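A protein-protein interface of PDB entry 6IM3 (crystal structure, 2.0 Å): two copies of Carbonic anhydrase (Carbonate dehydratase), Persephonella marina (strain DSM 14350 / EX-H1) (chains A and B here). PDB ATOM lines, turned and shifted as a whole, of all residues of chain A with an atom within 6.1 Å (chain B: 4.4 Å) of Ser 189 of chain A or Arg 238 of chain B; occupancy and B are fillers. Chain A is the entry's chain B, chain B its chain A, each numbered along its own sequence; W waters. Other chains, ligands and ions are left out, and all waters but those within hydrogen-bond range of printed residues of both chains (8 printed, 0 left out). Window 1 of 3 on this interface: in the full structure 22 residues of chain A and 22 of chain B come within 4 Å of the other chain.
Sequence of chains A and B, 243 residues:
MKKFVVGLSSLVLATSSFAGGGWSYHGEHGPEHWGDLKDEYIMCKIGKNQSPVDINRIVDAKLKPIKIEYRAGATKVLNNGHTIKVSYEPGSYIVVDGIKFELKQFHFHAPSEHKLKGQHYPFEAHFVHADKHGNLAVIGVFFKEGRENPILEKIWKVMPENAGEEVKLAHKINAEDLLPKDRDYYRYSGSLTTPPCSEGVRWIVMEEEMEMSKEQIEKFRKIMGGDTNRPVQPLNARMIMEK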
ATOM      1  N   ASN A  49      19.131  21.555  34.815  1.00  0.00           N
ATOM      2  CA  ASN A  49      18.533  22.875  34.839  1.00  0.00           C
ATOM      3  C   ASN A  49      17.352  22.989  35.792  1.00  0.00           C
ATOM      4  O   ASN A  49      16.268  23.455  35.455  1.00  0.00           O
ATOM      5  CB  ASN A  49      18.124  23.290  33.417  1.00  0.00           C
ATOM      6  CG  ASN A  49      19.340  23.374  32.477  1.00  0.00           C
ATOM      7  OD1 ASN A  49      20.032  24.379  32.450  1.00  0.00           O
ATOM      8  ND2 ASN A  49      19.634  22.313  31.771  1.00  0.00           N
ATOM      9  N   GLN A  50      17.617  22.552  37.016  1.00  0.00           N
ATOM     10  CA  GLN A  50      16.608  22.496  38.091  1.00  0.00           C
ATOM     11  C   GLN A  50      16.587  23.700  38.960  1.00  0.00           C
ATOM     12  O   GLN A  50      17.546  24.523  38.978  1.00  0.00           O
ATOM     13  CB  GLN A  50      16.873  21.260  38.994  1.00  0.00           C
ATOM     14  CG  GLN A  50      16.777  19.906  38.283  1.00  0.00           C
ATOM     15  CD  GLN A  50      15.315  19.528  38.119  1.00  0.00           C
ATOM     16  OE1 GLN A  50      14.641  19.198  39.120  1.00  0.00           O
ATOM     17  NE2 GLN A  50      14.802  19.607  36.889  1.00  0.00           N
ATOM     18  N   SER A  51      15.424  23.903  39.568  1.00  0.00           N
ATOM     19  CA  SER A  51      15.164  25.000  40.446  1.00  0.00           C
ATOM     20  C   SER A  51      14.772  24.387  41.853  1.00  0.00           C
ATOM     21  O   SER A  51      14.275  23.294  41.900  1.00  0.00           O
ATOM     22  CB  SER A  51      14.047  25.815  39.929  1.00  0.00           C
ATOM     23  OG  SER A  51      14.347  26.391  38.658  1.00  0.00           O
ATOM     24  N   ASP A  97       9.470  37.699  26.597  1.00  0.00           N
ATOM     25  CA  ASP A  97       9.946  37.338  25.197  1.00  0.00           C
ATOM     26  C   ASP A  97       8.821  37.542  24.179  1.00  0.00           C
ATOM     27  O   ASP A  97       8.649  36.763  23.252  1.00  0.00           O
ATOM     28  CB  ASP A  97      10.402  35.907  25.152  1.00  0.00           C
ATOM     29  CG  ASP A  97      11.504  35.588  26.200  1.00  0.00           C
ATOM     30  OD1 ASP A  97      12.309  36.511  26.465  1.00  0.00           O
ATOM     31  OD2 ASP A  97      11.658  34.376  26.587  1.00  0.00           O
ATOM     32  N   ARG A 187      16.733  36.607  36.125  1.00  0.00           N
ATOM     33  CA  ARG A 187      16.118  35.655  35.173  1.00  0.00           C
ATOM     34  C   ARG A 187      17.010  34.501  34.925  1.00  0.00           C
ATOM     35  O   ARG A 187      18.230  34.677  34.727  1.00  0.00           O
ATOM     36  CB  ARG A 187      15.714  36.353  33.893  1.00  0.00           C
ATOM     37  CG  ARG A 187      15.268  35.366  32.799  1.00  0.00           C
ATOM     38  CD  ARG A 187      14.669  36.012  31.590  1.00  0.00           C
ATOM     39  NE  ARG A 187      14.449  35.004  30.564  1.00  0.00           N
ATOM     40  CZ  ARG A 187      13.775  35.166  29.425  1.00  0.00           C
ATOM     41  NH1 ARG A 187      13.313  36.362  29.074  1.00  0.00           N
ATOM     42  NH2 ARG A 187      13.646  34.108  28.595  1.00  0.00           N
ATOM     43  N   TYR A 188      16.424  33.293  34.905  1.00  0.00           N
ATOM     44  CA  TYR A 188      17.150  32.124  34.473  1.00  0.00           C
ATOM     45  C   TYR A 188      16.172  31.051  33.995  1.00  0.00           C
ATOM     46  O   TYR A 188      14.970  31.165  34.141  1.00  0.00           O
ATOM     47  CB  TYR A 188      18.100  31.587  35.616  1.00  0.00           C
ATOM     48  CG  TYR A 188      17.371  30.874  36.741  1.00  0.00           C
ATOM     49  CD1 TYR A 188      16.756  31.579  37.758  1.00  0.00           C
ATOM     50  CD2 TYR A 188      17.308  29.493  36.777  1.00  0.00           C
ATOM     51  CE1 TYR A 188      16.099  30.905  38.777  1.00  0.00           C
ATOM     52  CE2 TYR A 188      16.674  28.822  37.817  1.00  0.00           C
ATOM     53  CZ  TYR A 188      16.049  29.541  38.787  1.00  0.00           C
ATOM     54  OH  TYR A 188      15.406  28.811  39.778  1.00  0.00           O
ATOM     55  N   SER A 189      16.731  30.074  33.324  1.00  0.00           N
ATOM     56  CA  SER A 189      16.008  28.908  32.790  1.00  0.00           C
ATOM     57  C   SER A 189      16.072  27.776  33.789  1.00  0.00           C
ATOM     58  O   SER A 189      17.168  27.276  34.143  1.00  0.00           O
ATOM     59  CB  SER A 189      16.622  28.441  31.502  1.00  0.00           C
ATOM     60  OG  SER A 189      16.086  27.252  31.017  1.00  0.00           O
ATOM     61  N   GLY A 190      14.917  27.375  34.263  1.00  0.00           N
ATOM     62  CA  GLY A 190      14.864  26.369  35.306  1.00  0.00           C
ATOM     63  C   GLY A 190      13.732  25.363  35.210  1.00  0.00           C
ATOM     64  O   GLY A 190      13.366  24.898  34.128  1.00  0.00           O
ATOM     65  N   SER A 191      13.174  25.029  36.363  1.00  0.00           N
ATOM     66  CA  SER A 191      12.226  23.884  36.511  1.00  0.00           C
ATOM     67  C   SER A 191      11.147  24.185  37.515  1.00  0.00           C
ATOM     68  O   SER A 191      11.229  25.132  38.304  1.00  0.00           O
ATOM     69  CB  SER A 191      12.896  22.597  36.937  1.00  0.00           C
ATOM     70  OG  SER A 191      13.171  22.527  38.356  1.00  0.00           O
ATOM     71  N   GLY A 200      12.357  23.744  31.236  1.00  0.00           N
ATOM     72  CA  GLY A 200      11.793  24.645  30.264  1.00  0.00           C
ATOM     73  C   GLY A 200      10.951  25.718  30.932  1.00  0.00           C
ATOM     74  O   GLY A 200      10.194  26.400  30.270  1.00  0.00           O
ATOM     75  N   VAL A 201      11.190  25.976  32.221  1.00  0.00           N
ATOM     76  CA  VAL A 201      10.465  27.019  32.934  1.00  0.00           C
ATOM     77  C   VAL A 201      11.229  28.327  32.987  1.00  0.00           C
ATOM     78  O   VAL A 201      12.386  28.373  33.413  1.00  0.00           O
ATOM     79  CB  VAL A 201      10.126  26.553  34.377  1.00  0.00           C
ATOM     80  CG1 VAL A 201       9.380  27.618  35.163  1.00  0.00           C
ATOM     81  CG2 VAL A 201       9.308  25.316  34.311  1.00  0.00           C
ATOM     82  N   ARG A 202      10.562  29.415  32.645  1.00  0.00           N
ATOM     83  CA  ARG A 202      11.148  30.762  32.786  1.00  0.00           C
ATOM     84  C   ARG A 202      10.992  31.220  34.222  1.00  0.00           C
ATOM     85  O   ARG A 202       9.837  31.409  34.661  1.00  0.00           O
ATOM     86  CB  ARG A 202      10.486  31.769  31.850  1.00  0.00           C
ATOM     87  CG  ARG A 202      10.790  31.535  30.370  1.00  0.00           C
ATOM     88  CD  ARG A 202       9.774  32.279  29.559  1.00  0.00           C
ATOM     89  NE  ARG A 202      10.127  32.459  28.135  1.00  0.00           N
ATOM     90  CZ  ARG A 202       9.786  31.660  27.135  1.00  0.00           C
ATOM     91  NH1 ARG A 202       9.245  30.499  27.362  1.00  0.00           N
ATOM     92  NH2 ARG A 202      10.136  31.981  25.878  1.00  0.00           N
ATOM     93  N   TRP A 203      12.111  31.471  34.892  1.00  0.00           N
ATOM     94  CA  TRP A 203      12.061  32.051  36.261  1.00  0.00           C
ATOM     95  C   TRP A 203      12.414  33.518  36.229  1.00  0.00           C
ATOM     96  O   TRP A 203      13.431  33.919  35.667  1.00  0.00           O
ATOM     97  CB  TRP A 203      13.009  31.295  37.189  1.00  0.00           C
ATOM     98  CG  TRP A 203      12.387  30.074  37.740  1.00  0.00           C
ATOM     99  CD1 TRP A 203      12.478  28.844  37.274  1.00  0.00           C
ATOM    100  CD2 TRP A 203      11.512  30.015  38.899  1.00  0.00           C
ATOM    101  NE1 TRP A 203      11.751  27.964  38.104  1.00  0.00           N
ATOM    102  CE2 TRP A 203      11.096  28.687  39.041  1.00  0.00           C
ATOM    103  CE3 TRP A 203      11.055  30.962  39.788  1.00  0.00           C
ATOM    104  CZ2 TRP A 203      10.313  28.260  40.087  1.00  0.00           C
ATOM    105  CZ3 TRP A 203      10.235  30.540  40.829  1.00  0.00           C
ATOM    106  CH2 TRP A 203       9.836  29.208  40.922  1.00  0.00           C
ATOM    107  N   ARG A 238      24.521  27.231  33.926  1.00  0.00           N
ATOM    108  CA  ARG A 238      23.749  28.441  33.908  1.00  0.00           C
ATOM    109  C   ARG A 238      24.358  29.652  34.579  1.00  0.00           C
ATOM    110  O   ARG A 238      25.180  29.550  35.482  1.00  0.00           O
ATOM    111  CB  ARG A 238      22.368  28.213  34.512  1.00  0.00           C
ATOM    112  CG  ARG A 238      21.516  27.178  33.769  1.00  0.00           C
ATOM    113  CD  ARG A 238      20.215  26.907  34.580  1.00  0.00           C
ATOM    114  NE  ARG A 238      20.535  26.116  35.769  1.00  0.00           N
ATOM    115  CZ  ARG A 238      19.645  25.714  36.648  1.00  0.00           C
ATOM    116  NH1 ARG A 238      18.366  26.059  36.499  1.00  0.00           N
ATOM    117  NH2 ARG A 238      20.020  24.939  37.673  1.00  0.00           N
ATOM    118  N   MET A 239      23.957  30.795  34.052  1.00  0.00           N
ATOM    119  CA  MET A 239      24.165  32.101  34.712  1.00  0.00           C
ATOM    120  C   MET A 239      22.823  32.692  35.065  1.00  0.00           C
ATOM    121  O   MET A 239      21.827  32.379  34.445  1.00  0.00           O
ATOM    122  CB  MET A 239      24.875  33.042  33.783  1.00  0.00           C
ATOM    123  CG  MET A 239      26.224  32.514  33.433  1.00  0.00           C
ATOM    124  SD  MET A 239      27.362  33.864  33.289  1.00  0.00           S
ATOM    125  CE  MET A 239      27.194  34.510  34.966  1.00  0.00           C
ATOM    126  N   LYS B  48      14.620  20.142  27.433  1.00  0.00           N
ATOM    127  CA  LYS B  48      14.214  21.499  27.115  1.00  0.00           C
ATOM    128  C   LYS B  48      15.359  22.522  26.970  1.00  0.00           C
ATOM    129  O   LYS B  48      15.100  23.723  26.800  1.00  0.00           O
ATOM    130  CB  LYS B  48      13.241  21.993  28.185  1.00  0.00           C
ATOM    131  CG  LYS B  48      11.983  21.121  28.357  1.00  0.00           C
ATOM    132  CD  LYS B  48      11.042  21.377  27.192  1.00  0.00           C
ATOM    133  CE  LYS B  48       9.714  20.671  27.424  1.00  0.00           C
ATOM    134  NZ  LYS B  48       8.677  21.290  26.561  1.00  0.00           N
ATOM    135  N   ASN B  49      16.585  22.048  27.145  1.00  0.00           N
ATOM    136  CA  ASN B  49      17.787  22.860  27.058  1.00  0.00           C
ATOM    137  C   ASN B  49      18.823  22.238  26.104  1.00  0.00           C
ATOM    138  O   ASN B  49      19.974  22.031  26.440  1.00  0.00           O
ATOM    139  CB  ASN B  49      18.381  23.078  28.459  1.00  0.00           C
ATOM    140  CG  ASN B  49      17.452  23.833  29.359  1.00  0.00           C
ATOM    141  OD1 ASN B  49      17.420  25.063  29.335  1.00  0.00           O
ATOM    142  ND2 ASN B  49      16.617  23.127  30.124  1.00  0.00           N
ATOM    143  N   GLN B  50      18.318  21.903  24.922  1.00  0.00           N
ATOM    144  CA  GLN B  50      19.077  21.241  23.889  1.00  0.00           C
ATOM    145  C   GLN B  50      19.768  22.199  22.937  1.00  0.00           C
ATOM    146  O   GLN B  50      19.430  23.371  22.835  1.00  0.00           O
ATOM    147  CB  GLN B  50      18.171  20.275  23.069  1.00  0.00           C
ATOM    148  CG  GLN B  50      17.564  19.124  23.873  1.00  0.00           C
ATOM    149  CD  GLN B  50      18.560  18.035  24.091  1.00  0.00           C
ATOM    150  OE1 GLN B  50      18.938  17.328  23.138  1.00  0.00           O
ATOM    151  NE2 GLN B  50      19.089  17.944  25.296  1.00  0.00           N
ATOM    152  N   VAL B  53      21.091  25.685  18.626  1.00  0.00           N
ATOM    153  CA  VAL B  53      19.943  26.594  18.571  1.00  0.00           C
ATOM    154  C   VAL B  53      20.140  27.611  17.462  1.00  0.00           C
ATOM    155  O   VAL B  53      21.269  27.875  17.029  1.00  0.00           O
ATOM    156  CB  VAL B  53      19.724  27.368  19.904  1.00  0.00           C
ATOM    157  CG1 VAL B  53      19.463  26.392  21.050  1.00  0.00           C
ATOM    158  CG2 VAL B  53      20.958  28.188  20.294  1.00  0.00           C
ATOM    159  N   ARG B  57      17.471  35.199  20.116  1.00  0.00           N
ATOM    160  CA  ARG B  57      16.926  35.916  21.276  1.00  0.00           C
ATOM    161  C   ARG B  57      18.132  36.230  22.120  1.00  0.00           C
ATOM    162  O   ARG B  57      18.554  35.459  22.942  1.00  0.00           O
ATOM    163  CB  ARG B  57      15.930  35.081  22.047  1.00  0.00           C
ATOM    164  CG  ARG B  57      15.219  35.809  23.156  1.00  0.00           C
ATOM    165  CD  ARG B  57      13.900  35.135  23.476  1.00  0.00           C
ATOM    166  NE  ARG B  57      14.071  33.852  24.101  1.00  0.00           N
ATOM    167  CZ  ARG B  57      13.144  32.919  24.134  1.00  0.00           C
ATOM    168  NH1 ARG B  57      11.994  33.123  23.573  1.00  0.00           N
ATOM    169  NH2 ARG B  57      13.374  31.796  24.730  1.00  0.00           N
ATOM    170  N   TYR B 188      25.240  30.350  26.267  1.00  0.00           N
ATOM    171  CA  TYR B 188      24.010  29.760  26.759  1.00  0.00           C
ATOM    172  C   TYR B 188      24.239  28.373  27.355  1.00  0.00           C
ATOM    173  O   TYR B 188      25.312  27.811  27.242  1.00  0.00           O
ATOM    174  CB  TYR B 188      22.900  29.783  25.666  1.00  0.00           C
ATOM    175  CG  TYR B 188      23.032  28.741  24.591  1.00  0.00           C
ATOM    176  CD1 TYR B 188      23.938  28.894  23.562  1.00  0.00           C
ATOM    177  CD2 TYR B 188      22.369  27.522  24.691  1.00  0.00           C
ATOM    178  CE1 TYR B 188      24.125  27.891  22.597  1.00  0.00           C
ATOM    179  CE2 TYR B 188      22.527  26.521  23.729  1.00  0.00           C
ATOM    180  CZ  TYR B 188      23.420  26.711  22.674  1.00  0.00           C
ATOM    181  OH  TYR B 188      23.548  25.728  21.770  1.00  0.00           O
ATOM    182  N   SER B 189      23.254  27.924  28.097  1.00  0.00           N
ATOM    183  CA  SER B 189      23.229  26.640  28.703  1.00  0.00           C
ATOM    184  C   SER B 189      22.509  25.606  27.830  1.00  0.00           C
ATOM    185  O   SER B 189      21.349  25.794  27.473  1.00  0.00           O
ATOM    186  CB  SER B 189      22.481  26.683  30.042  1.00  0.00           C
ATOM    187  OG  SER B 189      22.278  25.374  30.598  1.00  0.00           O
ATOM    188  N   GLY B 190      23.248  24.611  27.427  1.00  0.00           N
ATOM    189  CA  GLY B 190      22.748  23.651  26.405  1.00  0.00           C
ATOM    190  C   GLY B 190      23.143  22.225  26.594  1.00  0.00           C
ATOM    191  O   GLY B 190      23.221  21.724  27.717  1.00  0.00           O
ATOM    192  N   PRO B 234      14.447  24.140  20.011  1.00  0.00           N
ATOM    193  CA  PRO B 234      13.854  25.332  20.556  1.00  0.00           C
ATOM    194  C   PRO B 234      14.641  25.922  21.776  1.00  0.00           C
ATOM    195  O   PRO B 234      15.127  25.166  22.620  1.00  0.00           O
ATOM    196  CB  PRO B 234      12.474  24.831  21.053  1.00  0.00           C
ATOM    197  CG  PRO B 234      12.279  23.519  20.371  1.00  0.00           C
ATOM    198  CD  PRO B 234      13.610  22.947  20.177  1.00  0.00           C
ATOM    199  N   LEU B 235      14.570  27.237  21.926  1.00  0.00           N
ATOM    200  CA  LEU B 235      15.199  27.906  23.039  1.00  0.00           C
ATOM    201  C   LEU B 235      14.418  27.726  24.323  1.00  0.00           C
ATOM    202  O   LEU B 235      14.980  27.653  25.370  1.00  0.00           O
ATOM    203  CB  LEU B 235      15.327  29.385  22.747  1.00  0.00           C
ATOM    204  CG  LEU B 235      16.541  29.838  21.980  1.00  0.00           C
ATOM    205  CD1 LEU B 235      16.379  31.295  21.658  1.00  0.00           C
ATOM    206  CD2 LEU B 235      17.783  29.619  22.799  1.00  0.00           C
ATOM    207  N   ASN B 236      13.114  27.664  24.207  1.00  0.00           N
ATOM    208  CA  ASN B 236      12.254  27.492  25.347  1.00  0.00           C
ATOM    209  C   ASN B 236      12.407  28.651  26.325  1.00  0.00           C
ATOM    210  O   ASN B 236      12.166  29.754  25.955  1.00  0.00           O
ATOM    211  CB  ASN B 236      12.456  26.110  25.941  1.00  0.00           C
ATOM    212  CG  ASN B 236      11.912  25.005  25.051  1.00  0.00           C
ATOM    213  OD1 ASN B 236      10.877  25.134  24.449  1.00  0.00           O
ATOM    214  ND2 ASN B 236      12.608  23.925  24.989  1.00  0.00           N
ATOM    215  N   ALA B 237      12.776  28.406  27.561  1.00  0.00           N
ATOM    216  CA  ALA B 237      12.941  29.480  28.527  1.00  0.00           C
ATOM    217  C   ALA B 237      14.218  30.287  28.406  1.00  0.00           C
ATOM    218  O   ALA B 237      14.352  31.295  29.016  1.00  0.00           O
ATOM    219  CB  ALA B 237      12.840  28.938  29.923  1.00  0.00           C
ATOM    220  N   ARG B 238      15.170  29.780  27.523  1.00  0.00           N
ATOM    221  CA  ARG B 238      16.480  30.377  27.494  1.00  0.00           C
ATOM    222  C   ARG B 238      16.586  31.688  26.737  1.00  0.00           C
ATOM    223  O   ARG B 238      15.858  31.987  25.824  1.00  0.00           O
ATOM    224  CB  ARG B 238      17.519  29.362  26.935  1.00  0.00           C
ATOM    225  CG  ARG B 238      17.656  28.081  27.745  1.00  0.00           C
ATOM    226  CD  ARG B 238      18.516  27.094  27.027  1.00  0.00           C
ATOM    227  NE  ARG B 238      17.834  26.543  25.856  1.00  0.00           N
ATOM    228  CZ  ARG B 238      18.356  25.675  25.015  1.00  0.00           C
ATOM    229  NH1 ARG B 238      19.597  25.258  25.165  1.00  0.00           N
ATOM    230  NH2 ARG B 238      17.618  25.192  24.021  1.00  0.00           N
ATOM    231  N   MET B 239      17.555  32.457  27.182  1.00  0.00           N
ATOM    232  CA  MET B 239      18.085  33.613  26.443  1.00  0.00           C
ATOM    233  C   MET B 239      19.552  33.332  26.076  1.00  0.00           C
ATOM    234  O   MET B 239      20.222  32.571  26.732  1.00  0.00           O
ATOM    235  CB  MET B 239      18.068  34.745  27.410  1.00  0.00           C
ATOM    236  CG  MET B 239      18.422  36.160  26.791  1.00  0.00           C
ATOM    237  SD  MET B 239      16.961  37.062  26.185  1.00  0.00           S
ATOM    238  CE  MET B 239      16.016  36.864  27.675  1.00  0.00           C
HETATM  239  O   HOH W   1      14.568  25.908  28.523  1.00  0.00           O
HETATM  240  O   HOH W   2      19.323  26.465  30.767  1.00  0.00           O
HETATM  241  O   HOH W   3      21.886  22.636  29.783  1.00  0.00           O
HETATM  242  O   HOH W   4       9.995  34.878  21.876  1.00  0.00           O
HETATM  243  O   HOH W   5      16.112  32.442  30.866  1.00  0.00           O
HETATM  244  O   HOH W   6      15.013  24.689  32.003  1.00  0.00           O
HETATM  245  O   HOH W   7      22.964  23.603  33.222  1.00  0.00           O
HETATM  246  O   HOH W   8      10.210  30.385  23.355  1.00  0.00           O
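NH2 of Arg 202 of chain A lies close to NH1 of Arg 57 of chain B, at 3.2 Å.
The guanidinium group (NH2) of Arg 202 of chain A sits at hydrogen-bond distance from the backbone carbonyl oxygen (O) of Asn 236 of chain B (3.0 Å).
The backbone carbonyl oxygen (O) of Ala 237 of chain B lies within hydrogen-bond range of the guanidinium group (NH2) of Arg 187 of chain A, 2.9 Å away.
The side-chain hydroxyl of Ser 189 of chain A sits at hydrogen-bond distance from the side-chain amide oxygen of Asn 49 of chain B (3.1 Å).
OD1 of Asn 49 of chain A sits at hydrogen-bond distance from OG of Ser 189 of chain B, at 3.1 Å.
OD2 of Asp 97 of chain A is in salt-bridge range of NH1 of Arg 57 of chain B (3.3 Å).
Hydrophobic or aromatic side chains of chain B within 4 Å of the printed part of chain A: Ala 237 and Met 239.
Among the printed residues, merely in contact across the chains: Asn 49 of chain A with Asn 49 of chain B (3.5 Å), Asp 97 of chain A with Met 239 of chain B (3.9 Å), Arg 187 of chain A with Met 239 of chain B (3.1 Å), Ser 189 of chain A with Ala 237 of chain B (3.8 Å), Ser 189 of chain A with Arg 238 of chain B (3.7 Å), Gly 200 of chain A with Lys 48 of chain B (3.6 Å), Gly 200 of chain A with Ala 237 of chain B (3.7 Å), Val 201 of chain A with Ala 237 of chain B (3.5 Å), Arg 202 of chain A with Ala 237 of chain B (3.3 Å) and Arg 238 of chain A with Ser 189 of chain B (3.7 Å).
The backbone carbonyl oxygen (O) of Asn 49 of chain B lies close to the guanidinium group (NH1) of Arg 238 of chain B (3.5 Å).
NH2 of Arg 57 of chain B lies within hydrogen-bond range of O of Asn 236 of chain B (2.7 Å).
NE of Arg 238 of chain B lies within hydrogen-bond range of O of Leu 235 of chain B.
The backbone carbonyl oxygen of Ser 189 of chain A sits at hydrogen-bond distance from the guanidinium group of Arg 238 of chain A (2.9 Å).
The guanidinium group (NH1) of Arg 238 of chain B is in hydrogen-bond range of the backbone carbonyl oxygen (O) of Ser 189 of chain B (2.9 Å).
The backbone NH of Gly 200 of chain A lies within hydrogen-bond range of the backbone carbonyl oxygen of Gly 190 of chain A, 3.3 Å away.
Asn 49 of chain A touches its own counterpart, Asn 49 of chain B.
Asn 49 of chain A touches Ser 189 of chain B, and with the chains exchanged Ser 189 of chain A touches Asn 49 of chain B.
Ser 189 of chain A touches Arg 238 of chain B, and with the chains exchanged Arg 238 of chain A touches Ser 189 of chain B.
7 positions are printed for both chains.
Of chain A, only Ser 189 comes within 4 Å of Arg 238 of chain B.
Of the printed residues of chain B, Val 201 of chain A touches Ala 237 (3.5 Å).
Of the printed residues of chain B, Asp 97 of chain A touches Arg 57 and Met 239.
Of the printed residues of chain A, Arg 57 of chain B touches Asp 97 and Arg 202.
Printed residues of chain A within 4 Å of Ser 189 of chain B: Asn 49 (3.1 Å) and Arg 238 (3.7 Å).
Tyr 188 of chain A touches none of the printed residues of chain B.
The nearest printed residue of chain B that does not touch Ser 189 of chain A is Lys 48 of chain B (5.6 Å).
The nearest residue of chain A that does not touch Arg 238 of chain B is Arg 187 of chain A (4.1 Å).
Water W3 lies within hydrogen-bond range of O of Gly 190 of chain B, OG of Ser 189 of chain B and ND2 of Asn 49 of chain A.
Water W4 lies within hydrogen-bond range of the backbone carbonyl oxygen of Asp 97 of chain A (2.7 Å) and the guanidinium group of Arg 57 of chain B (3.2 Å).
Water W6 lies within hydrogen-bond range of the backbone carbonyl oxygen (O) of Gly 190 of chain A, the backbone NH (N) of Gly 200 of chain A, the side-chain amide nitrogen (ND2) of Asn 49 of chain B and the side-chain hydroxyl (OG) of Ser 189 of chain A.
Water W5 lies within hydrogen-bond range of the backbone carbonyl oxygen of Ala 237 of chain B (2.8 Å), the guanidinium group of Arg 187 of chain A (3.1 Å) and the backbone NH of Ser 189 of chain A (3.5 Å).
Water W8 lies within hydrogen-bond range of the guanidinium group of Arg 202 of chain A (3.0 Å), the guanidinium group of Arg 57 of chain B (3.3 Å) and the backbone carbonyl oxygen of Asn 236 of chain B (3.3 Å).
Water W7 bridges OD1 of Asn 49 of chain A (3.1 Å) and OG of Ser 189 of chain B (3.2 Å).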
